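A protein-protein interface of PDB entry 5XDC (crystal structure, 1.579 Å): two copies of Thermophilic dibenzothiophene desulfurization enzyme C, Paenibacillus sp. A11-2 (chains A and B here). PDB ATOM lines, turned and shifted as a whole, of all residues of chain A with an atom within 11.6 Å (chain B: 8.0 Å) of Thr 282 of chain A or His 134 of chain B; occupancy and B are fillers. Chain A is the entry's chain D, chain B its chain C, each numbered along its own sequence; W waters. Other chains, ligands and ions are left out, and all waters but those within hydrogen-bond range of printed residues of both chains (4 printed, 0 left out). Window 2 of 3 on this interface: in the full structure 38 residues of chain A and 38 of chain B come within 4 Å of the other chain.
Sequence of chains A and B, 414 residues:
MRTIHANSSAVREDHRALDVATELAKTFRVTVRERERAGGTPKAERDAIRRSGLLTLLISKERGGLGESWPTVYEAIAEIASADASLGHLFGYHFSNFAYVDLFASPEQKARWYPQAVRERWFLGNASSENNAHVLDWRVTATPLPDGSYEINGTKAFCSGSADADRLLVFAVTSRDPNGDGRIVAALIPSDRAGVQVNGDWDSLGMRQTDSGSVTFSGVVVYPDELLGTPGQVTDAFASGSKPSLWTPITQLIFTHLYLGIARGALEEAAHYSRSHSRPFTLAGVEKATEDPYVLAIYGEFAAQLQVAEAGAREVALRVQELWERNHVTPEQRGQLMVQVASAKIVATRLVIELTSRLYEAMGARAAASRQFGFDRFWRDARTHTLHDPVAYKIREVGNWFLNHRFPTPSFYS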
ATOM      1  N   SER A 278     -23.586  31.703   4.499  1.00  0.00           N
ATOM      2  CA  SER A 278     -24.277  30.496   4.914  1.00  0.00           C
ATOM      3  C   SER A 278     -23.338  29.307   4.773  1.00  0.00           C
ATOM      4  O   SER A 278     -22.592  29.203   3.794  1.00  0.00           O
ATOM      5  CB  SER A 278     -25.546  30.291   4.091  1.00  0.00           C
ATOM      6  OG  SER A 278     -26.521  31.248   4.454  1.00  0.00           O
ATOM      7  N   ARG A 279     -23.339  28.444   5.787  1.00  0.00           N
ATOM      8  CA  ARG A 279     -22.691  27.144   5.753  1.00  0.00           C
ATOM      9  C   ARG A 279     -23.684  26.097   5.272  1.00  0.00           C
ATOM     10  O   ARG A 279     -24.889  26.217   5.523  1.00  0.00           O
ATOM     11  CB  ARG A 279     -22.206  26.741   7.142  1.00  0.00           C
ATOM     12  CG  ARG A 279     -20.993  27.462   7.658  1.00  0.00           C
ATOM     13  CD  ARG A 279     -20.665  26.977   9.072  1.00  0.00           C
ATOM     14  NE  ARG A 279     -21.802  27.133   9.979  1.00  0.00           N
ATOM     15  CZ  ARG A 279     -21.810  26.755  11.253  1.00  0.00           C
ATOM     16  NH1 ARG A 279     -20.735  26.193  11.793  1.00  0.00           N
ATOM     17  NH2 ARG A 279     -22.897  26.939  11.992  1.00  0.00           N
ATOM     18  N   PRO A 280     -23.232  25.037   4.610  1.00  0.00           N
ATOM     19  CA  PRO A 280     -24.138  23.911   4.361  1.00  0.00           C
ATOM     20  C   PRO A 280     -24.472  23.210   5.666  1.00  0.00           C
ATOM     21  O   PRO A 280     -23.619  23.062   6.543  1.00  0.00           O
ATOM     22  CB  PRO A 280     -23.341  23.004   3.416  1.00  0.00           C
ATOM     23  CG  PRO A 280     -21.913  23.337   3.685  1.00  0.00           C
ATOM     24  CD  PRO A 280     -21.873  24.783   4.106  1.00  0.00           C
ATOM     25  N   PHE A 281     -25.732  22.792   5.807  1.00  0.00           N
ATOM     26  CA  PHE A 281     -26.086  21.969   6.957  1.00  0.00           C
ATOM     27  C   PHE A 281     -25.262  20.690   6.910  1.00  0.00           C
ATOM     28  O   PHE A 281     -25.129  20.065   5.853  1.00  0.00           O
ATOM     29  CB  PHE A 281     -27.581  21.647   6.967  1.00  0.00           C
ATOM     30  CG  PHE A 281     -28.023  20.817   8.150  1.00  0.00           C
ATOM     31  CD1 PHE A 281     -27.636  21.142   9.440  1.00  0.00           C
ATOM     32  CD2 PHE A 281     -28.850  19.726   7.969  1.00  0.00           C
ATOM     33  CE1 PHE A 281     -28.054  20.378  10.523  1.00  0.00           C
ATOM     34  CE2 PHE A 281     -29.270  18.971   9.042  1.00  0.00           C
ATOM     35  CZ  PHE A 281     -28.875  19.296  10.316  1.00  0.00           C
ATOM     36  N   THR A 282     -24.694  20.311   8.060  1.00  0.00           N
ATOM     37  CA  THR A 282     -23.712  19.231   8.073  1.00  0.00           C
ATOM     38  C   THR A 282     -24.302  17.921   7.565  1.00  0.00           C
ATOM     39  O   THR A 282     -23.579  17.103   6.986  1.00  0.00           O
ATOM     40  CB  THR A 282     -23.136  19.048   9.483  1.00  0.00           C
ATOM     41  OG1 THR A 282     -21.969  18.214   9.418  1.00  0.00           O
ATOM     42  CG2 THR A 282     -24.173  18.428  10.445  1.00  0.00           C
ATOM     43  N   LEU A 283     -25.598  17.696   7.770  1.00  0.00           N
ATOM     44  CA  LEU A 283     -26.236  16.476   7.283  1.00  0.00           C
ATOM     45  C   LEU A 283     -26.777  16.609   5.861  1.00  0.00           C
ATOM     46  O   LEU A 283     -27.402  15.667   5.363  1.00  0.00           O
ATOM     47  CB  LEU A 283     -27.376  16.059   8.222  1.00  0.00           C
ATOM     48  CG  LEU A 283     -27.042  15.894   9.711  1.00  0.00           C
ATOM     49  CD1 LEU A 283     -28.243  15.328  10.475  1.00  0.00           C
ATOM     50  CD2 LEU A 283     -25.823  15.000   9.903  1.00  0.00           C
ATOM     51  N   ALA A 284     -26.561  17.745   5.192  1.00  0.00           N
ATOM     52  CA  ALA A 284     -27.156  17.935   3.870  1.00  0.00           C
ATOM     53  C   ALA A 284     -26.468  17.105   2.794  1.00  0.00           C
ATOM     54  O   ALA A 284     -27.085  16.820   1.760  1.00  0.00           O
ATOM     55  CB  ALA A 284     -27.112  19.410   3.473  1.00  0.00           C
ATOM     56  N   GLY A 285     -25.214  16.712   3.002  1.00  0.00           N
ATOM     57  CA  GLY A 285     -24.480  16.090   1.920  1.00  0.00           C
ATOM     58  C   GLY A 285     -24.256  17.010   0.742  1.00  0.00           C
ATOM     59  O   GLY A 285     -23.996  16.540  -0.366  1.00  0.00           O
ATOM     60  N   VAL A 286     -24.367  18.318   0.945  1.00  0.00           N
ATOM     61  CA  VAL A 286     -24.032  19.285  -0.089  1.00  0.00           C
ATOM     62  C   VAL A 286     -22.850  20.103   0.411  1.00  0.00           C
ATOM     63  O   VAL A 286     -22.660  20.292   1.618  1.00  0.00           O
ATOM     64  CB  VAL A 286     -25.235  20.185  -0.463  1.00  0.00           C
ATOM     65  CG1 VAL A 286     -25.526  21.209   0.626  1.00  0.00           C
ATOM     66  CG2 VAL A 286     -25.006  20.851  -1.807  1.00  0.00           C
ATOM     67  N   GLU A 287     -22.037  20.570  -0.529  1.00  0.00           N
ATOM     68  CA  GLU A 287     -20.805  21.255  -0.174  1.00  0.00           C
ATOM     69  C   GLU A 287     -21.010  22.744   0.037  1.00  0.00           C
ATOM     70  O   GLU A 287     -20.268  23.356   0.815  1.00  0.00           O
ATOM     71  CB  GLU A 287     -19.751  21.022  -1.259  1.00  0.00           C
ATOM     72  CG  GLU A 287     -19.540  19.547  -1.607  1.00  0.00           C
ATOM     73  CD  GLU A 287     -18.695  19.351  -2.853  1.00  0.00           C
ATOM     74  OE1 GLU A 287     -17.768  20.159  -3.079  1.00  0.00           O
ATOM     75  OE2 GLU A 287     -18.966  18.391  -3.609  1.00  0.00           O
ATOM     76  N   LYS A 288     -22.002  23.338  -0.626  1.00  0.00           N
ATOM     77  CA  LYS A 288     -22.275  24.764  -0.521  1.00  0.00           C
ATOM     78  C   LYS A 288     -23.763  24.987  -0.300  1.00  0.00           C
ATOM     79  O   LYS A 288     -24.594  24.360  -0.964  1.00  0.00           O
ATOM     80  CB  LYS A 288     -21.823  25.518  -1.784  1.00  0.00           C
ATOM     81  CG  LYS A 288     -20.317  25.565  -1.984  1.00  0.00           C
ATOM     82  CD  LYS A 288     -19.892  26.815  -2.743  1.00  0.00           C
ATOM     83  CE  LYS A 288     -20.305  26.766  -4.209  1.00  0.00           C
ATOM     84  NZ  LYS A 288     -19.896  28.007  -4.935  1.00  0.00           N
ATOM     85  N   ALA A 289     -24.089  25.898   0.621  1.00  0.00           N
ATOM     86  CA  ALA A 289     -25.486  26.239   0.871  1.00  0.00           C
ATOM     87  C   ALA A 289     -26.179  26.744  -0.387  1.00  0.00           C
ATOM     88  O   ALA A 289     -27.387  26.554  -0.546  1.00  0.00           O
ATOM     89  CB  ALA A 289     -25.585  27.295   1.972  1.00  0.00           C
ATOM     90  N   ASP A 292     -27.837  23.923  -2.089  1.00  0.00           N
ATOM     91  CA  ASP A 292     -28.787  23.128  -1.322  1.00  0.00           C
ATOM     92  C   ASP A 292     -30.158  23.181  -1.989  1.00  0.00           C
ATOM     93  O   ASP A 292     -30.630  24.270  -2.331  1.00  0.00           O
ATOM     94  CB  ASP A 292     -28.853  23.666   0.103  1.00  0.00           C
ATOM     95  CG  ASP A 292     -29.797  22.877   0.980  1.00  0.00           C
ATOM     96  OD1 ASP A 292     -31.021  23.110   0.903  1.00  0.00           O
ATOM     97  OD2 ASP A 292     -29.319  22.003   1.729  1.00  0.00           O
ATOM     98  N   PRO A 293     -30.813  22.042  -2.224  1.00  0.00           N
ATOM     99  CA  PRO A 293     -32.077  22.081  -2.977  1.00  0.00           C
ATOM    100  C   PRO A 293     -33.170  22.870  -2.287  1.00  0.00           C
ATOM    101  O   PRO A 293     -34.041  23.446  -2.956  1.00  0.00           O
ATOM    102  CB  PRO A 293     -32.458  20.602  -3.093  1.00  0.00           C
ATOM    103  CG  PRO A 293     -31.777  19.945  -1.949  1.00  0.00           C
ATOM    104  CD  PRO A 293     -30.486  20.676  -1.780  1.00  0.00           C
ATOM    105  N   TYR A 294     -33.157  22.913  -0.958  1.00  0.00           N
ATOM    106  CA  TYR A 294     -34.235  23.582  -0.242  1.00  0.00           C
ATOM    107  C   TYR A 294     -33.981  25.073  -0.143  1.00  0.00           C
ATOM    108  O   TYR A 294     -34.928  25.866  -0.206  1.00  0.00           O
ATOM    109  CB  TYR A 294     -34.413  22.927   1.126  1.00  0.00           C
ATOM    110  CG  TYR A 294     -34.702  21.451   0.979  1.00  0.00           C
ATOM    111  CD1 TYR A 294     -35.725  21.017   0.157  1.00  0.00           C
ATOM    112  CD2 TYR A 294     -33.943  20.507   1.630  1.00  0.00           C
ATOM    113  CE1 TYR A 294     -35.991  19.680  -0.006  1.00  0.00           C
ATOM    114  CE2 TYR A 294     -34.204  19.157   1.475  1.00  0.00           C
ATOM    115  CZ  TYR A 294     -35.234  18.754   0.660  1.00  0.00           C
ATOM    116  OH  TYR A 294     -35.511  17.412   0.498  1.00  0.00           O
ATOM    117  N   VAL A 295     -32.712  25.474   0.001  1.00  0.00           N
ATOM    118  CA  VAL A 295     -32.352  26.881  -0.137  1.00  0.00           C
ATOM    119  C   VAL A 295     -32.764  27.391  -1.507  1.00  0.00           C
ATOM    120  O   VAL A 295     -33.386  28.454  -1.633  1.00  0.00           O
ATOM    121  CB  VAL A 295     -30.840  27.063   0.112  1.00  0.00           C
ATOM    122  CG1 VAL A 295     -30.376  28.463  -0.242  1.00  0.00           C
ATOM    123  CG2 VAL A 295     -30.502  26.750   1.567  1.00  0.00           C
ATOM    124  N   MET A 363     -31.065  31.263   5.137  1.00  0.00           N
ATOM    125  CA  MET A 363     -29.813  31.858   5.578  1.00  0.00           C
ATOM    126  C   MET A 363     -29.165  31.093   6.720  1.00  0.00           C
ATOM    127  O   MET A 363     -27.942  30.948   6.737  1.00  0.00           O
ATOM    128  CB  MET A 363     -30.036  33.313   6.007  1.00  0.00           C
ATOM    129  CG  MET A 363     -30.366  34.263   4.844  1.00  0.00           C
ATOM    130  SD  MET A 363     -30.419  35.971   5.355  1.00  0.00           S
ATOM    131  CE  MET A 363     -32.008  35.974   6.138  1.00  0.00           C
ATOM    132  N   GLY A 364     -29.949  30.601   7.669  1.00  0.00           N
ATOM    133  CA  GLY A 364     -29.440  29.806   8.770  1.00  0.00           C
ATOM    134  C   GLY A 364     -29.465  30.556  10.095  1.00  0.00           C
ATOM    135  O   GLY A 364     -29.782  31.742  10.180  1.00  0.00           O
ATOM    136  N   ALA A 365     -29.106  29.812  11.149  1.00  0.00           N
ATOM    137  CA  ALA A 365     -29.249  30.312  12.514  1.00  0.00           C
ATOM    138  C   ALA A 365     -28.414  31.565  12.762  1.00  0.00           C
ATOM    139  O   ALA A 365     -28.832  32.453  13.519  1.00  0.00           O
ATOM    140  CB  ALA A 365     -28.858  29.221  13.511  1.00  0.00           C
ATOM    141  N   ARG A 366     -27.222  31.651  12.164  1.00  0.00           N
ATOM    142  CA  ARG A 366     -26.350  32.785  12.470  1.00  0.00           C
ATOM    143  C   ARG A 366     -26.933  34.113  11.989  1.00  0.00           C
ATOM    144  O   ARG A 366     -26.579  35.163  12.533  1.00  0.00           O
ATOM    145  CB  ARG A 366     -24.961  32.577  11.870  1.00  0.00           C
ATOM    146  CG  ARG A 366     -24.084  31.617  12.680  1.00  0.00           C
ATOM    147  CD  ARG A 366     -22.733  31.429  12.011  1.00  0.00           C
ATOM    148  NE  ARG A 366     -22.878  30.812  10.695  1.00  0.00           N
ATOM    149  CZ  ARG A 366     -22.156  31.116   9.621  1.00  0.00           C
ATOM    150  NH1 ARG A 366     -21.218  32.056   9.667  1.00  0.00           N
ATOM    151  NH2 ARG A 366     -22.386  30.482   8.484  1.00  0.00           N
ATOM    152  N   ASN B 131     -22.769  21.040  17.215  1.00  0.00           N
ATOM    153  CA  ASN B 131     -21.647  21.176  16.287  1.00  0.00           C
ATOM    154  C   ASN B 131     -22.167  20.956  14.873  1.00  0.00           C
ATOM    155  O   ASN B 131     -22.410  19.818  14.462  1.00  0.00           O
ATOM    156  CB  ASN B 131     -20.551  20.171  16.615  1.00  0.00           C
ATOM    157  CG  ASN B 131     -19.996  20.351  18.003  1.00  0.00           C
ATOM    158  OD1 ASN B 131     -19.097  21.168  18.222  1.00  0.00           O
ATOM    159  ND2 ASN B 131     -20.527  19.593  18.956  1.00  0.00           N
ATOM    160  N   ASN B 132     -22.318  22.044  14.116  1.00  0.00           N
ATOM    161  CA  ASN B 132     -22.814  21.938  12.743  1.00  0.00           C
ATOM    162  C   ASN B 132     -21.647  21.634  11.799  1.00  0.00           C
ATOM    163  O   ASN B 132     -21.300  22.405  10.900  1.00  0.00           O
ATOM    164  CB  ASN B 132     -23.546  23.208  12.335  1.00  0.00           C
ATOM    165  CG  ASN B 132     -24.107  23.121  10.932  1.00  0.00           C
ATOM    166  OD1 ASN B 132     -24.385  22.027  10.432  1.00  0.00           O
ATOM    167  ND2 ASN B 132     -24.259  24.267  10.281  1.00  0.00           N
ATOM    168  N   ALA B 133     -21.042  20.468  12.009  1.00  0.00           N
ATOM    169  CA  ALA B 133     -19.854  20.101  11.248  1.00  0.00           C
ATOM    170  C   ALA B 133     -19.491  18.656  11.548  1.00  0.00           C
ATOM    171  O   ALA B 133     -19.853  18.110  12.593  1.00  0.00           O
ATOM    172  CB  ALA B 133     -18.671  21.014  11.577  1.00  0.00           C
ATOM    173  N   HIS B 134     -18.749  18.057  10.618  1.00  0.00           N
ATOM    174  CA  HIS B 134     -18.221  16.715  10.816  1.00  0.00           C
ATOM    175  C   HIS B 134     -17.232  16.691  11.981  1.00  0.00           C
ATOM    176  O   HIS B 134     -16.590  17.695  12.308  1.00  0.00           O
ATOM    177  CB  HIS B 134     -17.555  16.220   9.530  1.00  0.00           C
ATOM    178  CG  HIS B 134     -18.456  16.275   8.335  1.00  0.00           C
ATOM    179  ND1 HIS B 134     -19.566  15.467   8.202  1.00  0.00           N
ATOM    180  CD2 HIS B 134     -18.426  17.056   7.228  1.00  0.00           C
ATOM    181  CE1 HIS B 134     -20.175  15.742   7.062  1.00  0.00           C
ATOM    182  NE2 HIS B 134     -19.505  16.703   6.453  1.00  0.00           N
ATOM    183  N   VAL B 135     -17.113  15.512  12.598  1.00  0.00           N
ATOM    184  CA  VAL B 135     -16.391  15.372  13.863  1.00  0.00           C
ATOM    185  C   VAL B 135     -14.954  15.864  13.729  1.00  0.00           C
ATOM    186  O   VAL B 135     -14.418  16.512  14.637  1.00  0.00           O
ATOM    187  CB  VAL B 135     -16.455  13.908  14.336  1.00  0.00           C
ATOM    188  CG1 VAL B 135     -15.568  13.675  15.547  1.00  0.00           C
ATOM    189  CG2 VAL B 135     -17.903  13.533  14.651  1.00  0.00           C
ATOM    190  N   LEU B 136     -14.304  15.565  12.607  1.00  0.00           N
ATOM    191  CA  LEU B 136     -12.915  15.978  12.453  1.00  0.00           C
ATOM    192  C   LEU B 136     -12.764  17.481  12.270  1.00  0.00           C
ATOM    193  O   LEU B 136     -11.636  17.980  12.322  1.00  0.00           O
ATOM    194  CB  LEU B 136     -12.271  15.234  11.279  1.00  0.00           C
ATOM    195  CG  LEU B 136     -12.000  13.758  11.584  1.00  0.00           C
ATOM    196  CD1 LEU B 136     -11.746  12.957  10.310  1.00  0.00           C
ATOM    197  CD2 LEU B 136     -10.823  13.616  12.552  1.00  0.00           C
ATOM    198  N   ASP B 137     -13.860  18.215  12.085  1.00  0.00           N
ATOM    199  CA  ASP B 137     -13.809  19.663  11.956  1.00  0.00           C
ATOM    200  C   ASP B 137     -14.303  20.392  13.205  1.00  0.00           C
ATOM    201  O   ASP B 137     -14.451  21.619  13.175  1.00  0.00           O
ATOM    202  CB  ASP B 137     -14.621  20.098  10.733  1.00  0.00           C
ATOM    203  CG  ASP B 137     -14.074  19.516   9.440  1.00  0.00           C
ATOM    204  OD1 ASP B 137     -12.839  19.376   9.328  1.00  0.00           O
ATOM    205  OD2 ASP B 137     -14.880  19.193   8.541  1.00  0.00           O
ATOM    206  N   TRP B 138     -14.551  19.678  14.302  1.00  0.00           N
ATOM    207  CA  TRP B 138     -15.052  20.319  15.512  1.00  0.00           C
ATOM    208  C   TRP B 138     -14.018  21.281  16.083  1.00  0.00           C
ATOM    209  O   TRP B 138     -12.807  21.067  15.981  1.00  0.00           O
ATOM    210  CB  TRP B 138     -15.423  19.282  16.569  1.00  0.00           C
ATOM    211  CG  TRP B 138     -16.706  18.589  16.299  1.00  0.00           C
ATOM    212  CD1 TRP B 138     -17.353  18.497  15.100  1.00  0.00           C
ATOM    213  CD2 TRP B 138     -17.513  17.884  17.248  1.00  0.00           C
ATOM    214  NE1 TRP B 138     -18.514  17.773  15.244  1.00  0.00           N
ATOM    215  CE2 TRP B 138     -18.636  17.387  16.554  1.00  0.00           C
ATOM    216  CE3 TRP B 138     -17.397  17.625  18.619  1.00  0.00           C
ATOM    217  CZ2 TRP B 138     -19.635  16.647  17.183  1.00  0.00           C
ATOM    218  CZ3 TRP B 138     -18.392  16.892  19.244  1.00  0.00           C
ATOM    219  CH2 TRP B 138     -19.496  16.411  18.526  1.00  0.00           C
ATOM    220  N   ARG B 139     -14.519  22.357  16.702  1.00  0.00           N
ATOM    221  CA  ARG B 139     -13.652  23.457  17.113  1.00  0.00           C
ATOM    222  C   ARG B 139     -12.787  23.096  18.317  1.00  0.00           C
ATOM    223  O   ARG B 139     -11.699  23.654  18.485  1.00  0.00           O
ATOM    224  CB  ARG B 139     -14.501  24.693  17.430  1.00  0.00           C
ATOM    225  N   VAL B 173     -13.143  16.622  20.517  1.00  0.00           N
ATOM    226  CA  VAL B 173     -12.683  15.520  19.676  1.00  0.00           C
ATOM    227  C   VAL B 173     -11.226  15.238  20.011  1.00  0.00           C
ATOM    228  O   VAL B 173     -10.420  16.163  20.158  1.00  0.00           O
ATOM    229  CB  VAL B 173     -12.865  15.827  18.173  1.00  0.00           C
ATOM    230  CG1 VAL B 173     -12.112  17.075  17.763  1.00  0.00           C
ATOM    231  CG2 VAL B 173     -12.432  14.659  17.332  1.00  0.00           C
ATOM    232  N   ILE B 184     -15.227  11.413  19.904  1.00  0.00           N
ATOM    233  CA  ILE B 184     -15.971  12.424  20.659  1.00  0.00           C
ATOM    234  C   ILE B 184     -15.883  12.115  22.146  1.00  0.00           C
ATOM    235  O   ILE B 184     -16.272  11.030  22.592  1.00  0.00           O
ATOM    236  CB  ILE B 184     -17.438  12.495  20.210  1.00  0.00           C
ATOM    237  CG1 ILE B 184     -17.521  13.001  18.774  1.00  0.00           C
ATOM    238  CG2 ILE B 184     -18.233  13.427  21.128  1.00  0.00           C
ATOM    239  CD1 ILE B 184     -18.886  12.861  18.152  1.00  0.00           C
ATOM    240  N   PRO B 390     -32.236  22.852  10.302  1.00  0.00           N
ATOM    241  CA  PRO B 390     -33.187  23.281   9.263  1.00  0.00           C
ATOM    242  C   PRO B 390     -34.404  22.366   9.197  1.00  0.00           C
ATOM    243  O   PRO B 390     -34.287  21.143   9.090  1.00  0.00           O
ATOM    244  CB  PRO B 390     -32.363  23.231   7.970  1.00  0.00           C
ATOM    245  CG  PRO B 390     -31.190  22.412   8.262  1.00  0.00           C
ATOM    246  CD  PRO B 390     -30.940  22.448   9.740  1.00  0.00           C
ATOM    247  N   TYR B 393     -34.794  19.611   6.516  1.00  0.00           N
ATOM    248  CA  TYR B 393     -34.228  18.279   6.660  1.00  0.00           C
ATOM    249  C   TYR B 393     -35.011  17.426   7.647  1.00  0.00           C
ATOM    250  O   TYR B 393     -35.018  16.200   7.512  1.00  0.00           O
ATOM    251  CB  TYR B 393     -32.728  18.393   6.997  1.00  0.00           C
ATOM    252  CG  TYR B 393     -31.997  18.739   5.724  1.00  0.00           C
ATOM    253  CD1 TYR B 393     -31.699  17.757   4.800  1.00  0.00           C
ATOM    254  CD2 TYR B 393     -31.712  20.052   5.391  1.00  0.00           C
ATOM    255  CE1 TYR B 393     -31.096  18.054   3.609  1.00  0.00           C
ATOM    256  CE2 TYR B 393     -31.096  20.368   4.196  1.00  0.00           C
ATOM    257  CZ  TYR B 393     -30.795  19.362   3.306  1.00  0.00           C
ATOM    258  OH  TYR B 393     -30.208  19.644   2.096  1.00  0.00           O
ATOM    259  N   SER B 411     -28.003  11.025  15.020  1.00  0.00           N
ATOM    260  CA  SER B 411     -26.927  12.002  15.094  1.00  0.00           C
ATOM    261  C   SER B 411     -27.283  12.980  16.212  1.00  0.00           C
ATOM    262  O   SER B 411     -28.248  12.767  16.952  1.00  0.00           O
ATOM    263  CB  SER B 411     -26.749  12.720  13.758  1.00  0.00           C
ATOM    264  OG  SER B 411     -27.821  13.627  13.561  1.00  0.00           O
ATOM    265  N   PHE B 412     -26.513  14.066  16.332  1.00  0.00           N
ATOM    266  CA  PHE B 412     -26.887  15.107  17.279  1.00  0.00           C
ATOM    267  C   PHE B 412     -28.066  15.943  16.797  1.00  0.00           C
ATOM    268  O   PHE B 412     -28.558  16.780  17.558  1.00  0.00           O
ATOM    269  CB  PHE B 412     -25.685  16.009  17.567  1.00  0.00           C
ATOM    270  CG  PHE B 412     -24.670  15.369  18.470  1.00  0.00           C
ATOM    271  CD1 PHE B 412     -24.841  15.389  19.839  1.00  0.00           C
ATOM    272  CD2 PHE B 412     -23.570  14.716  17.947  1.00  0.00           C
ATOM    273  CE1 PHE B 412     -23.918  14.788  20.685  1.00  0.00           C
ATOM    274  CE2 PHE B 412     -22.641  14.109  18.786  1.00  0.00           C
ATOM    275  CZ  PHE B 412     -22.822  14.150  20.153  1.00  0.00           C
ATOM    276  N   TYR B 413     -28.539  15.720  15.571  1.00  0.00           N
ATOM    277  CA  TYR B 413     -29.655  16.463  15.018  1.00  0.00           C
ATOM    278  C   TYR B 413     -30.789  15.586  14.519  1.00  0.00           C
ATOM    279  O   TYR B 413     -31.836  16.125  14.147  1.00  0.00           O
ATOM    280  CB  TYR B 413     -29.178  17.332  13.850  1.00  0.00           C
ATOM    281  CG  TYR B 413     -28.230  18.422  14.253  1.00  0.00           C
ATOM    282  CD1 TYR B 413     -28.705  19.577  14.838  1.00  0.00           C
ATOM    283  CD2 TYR B 413     -26.857  18.305  14.051  1.00  0.00           C
ATOM    284  CE1 TYR B 413     -27.855  20.597  15.211  1.00  0.00           C
ATOM    285  CE2 TYR B 413     -25.995  19.330  14.423  1.00  0.00           C
ATOM    286  CZ  TYR B 413     -26.510  20.471  15.008  1.00  0.00           C
ATOM    287  OH  TYR B 413     -25.698  21.513  15.387  1.00  0.00           O
HETATM  288  O   HOH W   1     -29.389  17.708   0.408  1.00  0.00           O
HETATM  289  O   HOH W   2     -25.782  25.406   8.251  1.00  0.00           O
HETATM  290  O   HOH W   3     -22.037  15.575   9.911  1.00  0.00           O
HETATM  291  O   HOH W   4     -21.503  22.461   8.066  1.00  0.00           O
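Water W4 bridges the backbone carbonyl oxygen (O) of Pro 280 of chain A (2.7 Å) and the backbone carbonyl oxygen (O) of Asn 132 of chain B (2.8 Å). Water W3 bridges the side-chain hydroxyl of Thr 282 of chain A (2.7 Å) and a ring nitrogen (ND1) of His 134 of chain B (3.0 Å). Water W1 lies within hydrogen-bond range of OH of Tyr 393 of chain B and O of Ala 284 of chain A. Water W2 bridges the side-chain amide nitrogen of Asn 132 of chain B (2.8 Å) and the backbone carbonyl oxygen of Arg 279 of chain A (3.0 Å).
The indole nitrogen of Trp 138 of chain B lies within hydrogen-bond range of the backbone carbonyl oxygen of Ala 133 of chain B (3.0 Å). The side-chain hydroxyl (OG) of Ser 411 of chain B lies within hydrogen-bond range of the backbone NH (N) of Tyr 413 of chain B (3.0 Å). The side-chain carboxylate (OD1) of Asp 292 of chain A sits at hydrogen-bond distance from the backbone NH (N) of Tyr 294 of chain A (2.8 Å). OD1 of Asp 292 of chain A lies within hydrogen-bond range of N of Val 295 of chain A, at 3.0 Å.
No position is printed for both chains.
Hydrophobic or aromatic side chains of chain B within 4 Å of the printed part of chain A: His 134, Pro 390 and Tyr 393. Of the 20 printed residues of chain A, 8 touch a printed residue of chain B. Among the printed residues, 12 pairs touch across the chains.
Of the printed residues of chain B, Arg 279 of chain A touches Asn 132 (3.5 Å). Thr 282 of chain A touches just these residues of chain B: Asn 132 (2.9 Å), Ala 133 (3.3 Å) and His 134 (3.4 Å). Gly 285 of chain A touches none of the printed residues of chain B. Arg 366 of chain A touches none of the printed residues of chain B. Of chain A, only Thr 282 comes within 4 Å of Ala 133 of chain B. His 134 of chain B touches one residue of chain A. No residue of chain A comes within 4 Å of Val 135 of chain B. No residue of chain A comes within 4 Å of Leu 136 of chain B. No residue of chain A comes within 4 Å of Asp 137 of chain B. No residue of chain A comes within 4 Å of Trp 138 of chain B. Printed residues of chain A within 4 Å of Tyr 393 of chain B: Phe 281, Ala 284, Asp 292 and Tyr 294. The nearest residue of chain A that does not touch His 134 of chain B is Leu 283 of chain A (5.8 Å).
ND2 of Asn 132 of chain B lies close to NH2 of Arg 279 of chain A, at 3.5 Å. The backbone NH (N) of Thr 282 of chain A sits at hydrogen-bond distance from the side-chain amide oxygen (OD1) of Asn 132 of chain B (2.9 Å). The backbone NH (N) of His 134 of chain B lies within hydrogen-bond range of the side-chain hydroxyl (OG1) of Thr 282 of chain A. The side-chain carboxylate of Asp 292 of chain A lies within hydrogen-bond range of the side-chain hydroxyl of Tyr 393 of chain B (2.5 Å).
Pro 280 of chain A touches Asn 132 of chain B (O to ND2, 3.98 Å). Phe 281 of chain A touches Asn 132 of chain B. CG of Phe 281 of chain A touches CG of Pro 390 of chain B, at 3.5 Å. CD2 of Phe 281 of chain A touches CD2 of Tyr 393 of chain B, 3.9 Å away. Ala 133 of chain B touches Thr 282 of chain A. Ser 411 of chain B touches Leu 283 of chain A (OG to CD1, 3.5 Å). Tyr 393 of chain B touches Ala 284 of chain A (OH to CB, 3.4 Å). Tyr 393 of chain B touches Tyr 294 of chain A.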
